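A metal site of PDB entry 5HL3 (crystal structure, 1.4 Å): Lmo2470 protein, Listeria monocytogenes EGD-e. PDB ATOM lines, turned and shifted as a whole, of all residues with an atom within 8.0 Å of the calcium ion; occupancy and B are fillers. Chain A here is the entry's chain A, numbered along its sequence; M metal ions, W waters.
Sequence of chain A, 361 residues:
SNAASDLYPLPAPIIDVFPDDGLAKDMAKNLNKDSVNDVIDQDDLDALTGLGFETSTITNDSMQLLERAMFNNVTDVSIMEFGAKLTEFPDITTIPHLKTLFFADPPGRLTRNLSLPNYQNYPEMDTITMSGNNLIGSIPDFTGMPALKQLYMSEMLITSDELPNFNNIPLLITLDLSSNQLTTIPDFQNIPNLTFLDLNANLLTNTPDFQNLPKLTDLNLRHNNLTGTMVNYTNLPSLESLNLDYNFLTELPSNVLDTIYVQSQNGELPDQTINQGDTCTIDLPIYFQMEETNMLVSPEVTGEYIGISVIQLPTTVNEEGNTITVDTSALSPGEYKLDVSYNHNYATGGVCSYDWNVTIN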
ATOM      1  N   ALA A 104     -11.533 -11.374 -31.866  1.00  0.00           N
ATOM      2  CA  ALA A 104     -12.324 -10.875 -30.774  1.00  0.00           C
ATOM      3  C   ALA A 104     -13.326 -11.898 -30.271  1.00  0.00           C
ATOM      4  O   ALA A 104     -13.675 -12.837 -30.974  1.00  0.00           O
ATOM      5  CB  ALA A 104     -13.066  -9.589 -31.177  1.00  0.00           C
ATOM      6  N   ASP A 105     -13.770 -11.677 -29.038  1.00  0.00           N
ATOM      7  CA  ASP A 105     -14.866 -12.397 -28.408  1.00  0.00           C
ATOM      8  C   ASP A 105     -16.131 -11.582 -28.768  1.00  0.00           C
ATOM      9  O   ASP A 105     -16.326 -10.491 -28.233  1.00  0.00           O
ATOM     10  CB  ASP A 105     -14.646 -12.397 -26.889  1.00  0.00           C
ATOM     11  CG  ASP A 105     -15.719 -13.130 -26.133  1.00  0.00           C
ATOM     12  OD1 ASP A 105     -16.764 -13.517 -26.706  1.00  0.00           O
ATOM     13  OD2 ASP A 105     -15.470 -13.249 -24.891  1.00  0.00           O
ATOM     14  N   PRO A 106     -16.935 -12.055 -29.703  1.00  0.00           N
ATOM     15  CA  PRO A 106     -18.081 -11.261 -30.132  1.00  0.00           C
ATOM     16  C   PRO A 106     -19.145 -11.162 -29.063  1.00  0.00           C
ATOM     17  O   PRO A 106     -19.153 -11.947 -28.119  1.00  0.00           O
ATOM     18  CB  PRO A 106     -18.617 -12.031 -31.361  1.00  0.00           C
ATOM     19  CG  PRO A 106     -17.569 -13.014 -31.729  1.00  0.00           C
ATOM     20  CD  PRO A 106     -16.841 -13.324 -30.479  1.00  0.00           C
ATOM     21  N   PRO A 107     -20.092 -10.236 -29.249  1.00  0.00           N
ATOM     22  CA  PRO A 107     -21.225 -10.183 -28.335  1.00  0.00           C
ATOM     23  C   PRO A 107     -21.988 -11.506 -28.306  1.00  0.00           C
ATOM     24  O   PRO A 107     -21.974 -12.270 -29.299  1.00  0.00           O
ATOM     25  CB  PRO A 107     -22.105  -9.089 -28.903  1.00  0.00           C
ATOM     26  CG  PRO A 107     -21.264  -8.300 -29.791  1.00  0.00           C
ATOM     27  CD  PRO A 107     -20.129  -9.179 -30.267  1.00  0.00           C
ATOM     28  N   GLY A 108     -22.685 -11.755 -27.214  1.00  0.00           N
ATOM     29  CA  GLY A 108     -23.408 -12.983 -27.072  1.00  0.00           C
ATOM     30  C   GLY A 108     -22.466 -14.115 -26.656  1.00  0.00           C
ATOM     31  O   GLY A 108     -21.268 -13.908 -26.359  1.00  0.00           O
ATOM     32  N   ARG A 109     -23.050 -15.308 -26.653  1.00  0.00           N
ATOM     33  CA  ARG A 109     -22.351 -16.487 -26.202  1.00  0.00           C
ATOM     34  C   ARG A 109     -22.133 -17.460 -27.346  1.00  0.00           C
ATOM     35  O   ARG A 109     -23.101 -17.932 -27.922  1.00  0.00           O
ATOM     36  CB  ARG A 109     -23.264 -17.155 -25.155  1.00  0.00           C
ATOM     37  CG  ARG A 109     -22.603 -18.175 -24.289  1.00  0.00           C
ATOM     38  CD  ARG A 109     -23.262 -18.183 -22.937  1.00  0.00           C
ATOM     39  NE  ARG A 109     -24.463 -19.001 -22.926  1.00  0.00           N
ATOM     40  CZ  ARG A 109     -25.725 -18.579 -23.051  1.00  0.00           C
ATOM     41  NH1 ARG A 109     -26.048 -17.287 -23.212  1.00  0.00           N
ATOM     42  NH2 ARG A 109     -26.687 -19.468 -23.001  1.00  0.00           N
ATOM     43  N   LEU A 110     -20.862 -17.730 -27.687  1.00  0.00           N
ATOM     44  CA  LEU A 110     -20.562 -18.751 -28.679  1.00  0.00           C
ATOM     45  C   LEU A 110     -21.280 -18.574 -30.007  1.00  0.00           C
ATOM     46  O   LEU A 110     -21.712 -19.533 -30.636  1.00  0.00           O
ATOM     47  CB  LEU A 110     -20.841 -20.167 -28.081  1.00  0.00           C
ATOM     48  CG  LEU A 110     -19.937 -20.547 -26.892  1.00  0.00           C
ATOM     49  CD1 LEU A 110     -20.525 -21.616 -25.967  1.00  0.00           C
ATOM     50  CD2 LEU A 110     -18.546 -20.961 -27.391  1.00  0.00           C
ATOM     51  N   THR A 111     -21.400 -17.314 -30.460  1.00  0.00           N
ATOM     52  CA  THR A 111     -22.165 -17.034 -31.667  1.00  0.00           C
ATOM     53  C   THR A 111     -21.402 -17.319 -32.953  1.00  0.00           C
ATOM     54  O   THR A 111     -21.992 -17.306 -34.040  1.00  0.00           O
ATOM     55  CB  THR A 111     -22.568 -15.561 -31.719  1.00  0.00           C
ATOM     56  OG1 THR A 111     -21.387 -14.772 -31.645  1.00  0.00           O
ATOM     57  CG2 THR A 111     -23.509 -15.213 -30.543  1.00  0.00           C
ATOM     58  N   ARG A 112     -20.071 -17.459 -32.873  1.00  0.00           N
ATOM     59  CA  ARG A 112     -19.231 -17.700 -34.050  1.00  0.00           C
ATOM     60  C   ARG A 112     -18.387 -18.950 -33.854  1.00  0.00           C
ATOM     61  O   ARG A 112     -18.063 -19.307 -32.756  1.00  0.00           O
ATOM     62  CB  ARG A 112     -18.313 -16.498 -34.304  1.00  0.00           C
ATOM     63  CG  ARG A 112     -19.002 -15.195 -34.675  1.00  0.00           C
ATOM     64  CD  ARG A 112     -19.466 -15.179 -36.122  1.00  0.00           C
ATOM     65  NE  ARG A 112     -20.148 -13.927 -36.433  1.00  0.00           N
ATOM     66  CZ  ARG A 112     -21.433 -13.693 -36.268  1.00  0.00           C
ATOM     67  NH1 ARG A 112     -22.243 -14.665 -35.872  1.00  0.00           N
ATOM     68  NH2 ARG A 112     -21.939 -12.482 -36.559  1.00  0.00           N
ATOM     69  N   SER A 131     -10.534 -16.806 -27.832  1.00  0.00           N
ATOM     70  CA  SER A 131     -11.556 -16.957 -26.780  1.00  0.00           C
ATOM     71  C   SER A 131     -12.935 -16.437 -27.149  1.00  0.00           C
ATOM     72  O   SER A 131     -13.105 -15.367 -27.714  1.00  0.00           O
ATOM     73  CB  SER A 131     -11.099 -16.243 -25.530  1.00  0.00           C
ATOM     74  OG  SER A 131      -9.848 -16.762 -25.103  1.00  0.00           O
ATOM     75  N   GLY A 132     -13.945 -17.232 -26.781  1.00  0.00           N
ATOM     76  CA  GLY A 132     -15.381 -16.878 -26.967  1.00  0.00           C
ATOM     77  C   GLY A 132     -16.010 -17.463 -28.202  1.00  0.00           C
ATOM     78  O   GLY A 132     -17.200 -17.350 -28.392  1.00  0.00           O
ATOM     79  N   ASN A 133     -15.201 -18.088 -29.040  1.00  0.00           N
ATOM     80  CA  ASN A 133     -15.655 -18.644 -30.304  1.00  0.00           C
ATOM     81  C   ASN A 133     -15.638 -20.167 -30.238  1.00  0.00           C
ATOM     82  O   ASN A 133     -14.728 -20.772 -29.665  1.00  0.00           O
ATOM     83  CB  ASN A 133     -14.755 -18.100 -31.402  1.00  0.00           C
ATOM     84  CG  ASN A 133     -14.824 -16.587 -31.477  1.00  0.00           C
ATOM     85  OD1 ASN A 133     -15.858 -16.040 -31.815  1.00  0.00           O
ATOM     86  ND2 ASN A 133     -13.739 -15.894 -31.116  1.00  0.00           N
ATOM     87  N   GLU A 155     -13.638 -20.447 -23.314  1.00  0.00           N
ATOM     88  CA  GLU A 155     -15.032 -20.434 -23.827  1.00  0.00           C
ATOM     89  C   GLU A 155     -15.092 -20.764 -25.306  1.00  0.00           C
ATOM     90  O   GLU A 155     -15.537 -19.954 -26.140  1.00  0.00           O
ATOM     91  CB  GLU A 155     -15.749 -19.100 -23.537  1.00  0.00           C
ATOM     92  CG  GLU A 155     -17.252 -19.275 -23.666  1.00  0.00           C
ATOM     93  CD  GLU A 155     -18.031 -18.035 -23.404  1.00  0.00           C
ATOM     94  OE1 GLU A 155     -17.754 -16.991 -24.019  1.00  0.00           O
ATOM     95  OE2 GLU A 155     -18.983 -18.109 -22.595  1.00  0.00           O
HETATM   96 CA    CA M   1     -19.048 -13.736 -26.585  1.00  0.00          CA
HETATM   97  O   HOH W   1     -19.219 -11.718 -25.140  1.00  0.00           O
HETATM   98  O   HOH W   2     -19.006 -14.519 -24.262  1.00  0.00           O
HETATM   99  O   HOH W   3     -19.923 -14.729 -28.896  1.00  0.00           O
HETATM  100  O   HOH W   4     -18.687 -16.184 -26.543  1.00  0.00           O
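Within 4 Å of the calcium ion: Asp 105, Pro 106 and Gly 108.
The nearest printed residue that does not touch the calcium ion is Pro 107 (4.1 Å).
O of Gly 108 is bound to the calcium ion (2.2 Å).
The calcium ion is bound by OD1 of Asp 105.
O of Pro 106 is bound to the calcium ion, at 2.4 Å.
Water W2 binds the calcium ion (2.5 Å).
The calcium ion is bound by water W4 (2.5 Å).
The calcium ion is bound by water W1, 2.5 Å away.
The calcium ion is bound by water W3 (2.7 Å).
The calcium ion has seven donor atoms within binding distance.
Water W4 lies within hydrogen-bond range of the backbone carbonyl oxygen of Gly 132 (2.6 Å), the side-chain carboxylate of Glu 155 (2.8 Å) and the backbone NH of Leu 110 (2.9 Å).
Water W3 lies within hydrogen-bond range of the side-chain hydroxyl of Thr 111 (3.1 Å), the backbone carbonyl oxygen of Pro 107 (3.2 Å) and the backbone NH of Leu 110 (3.4 Å).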
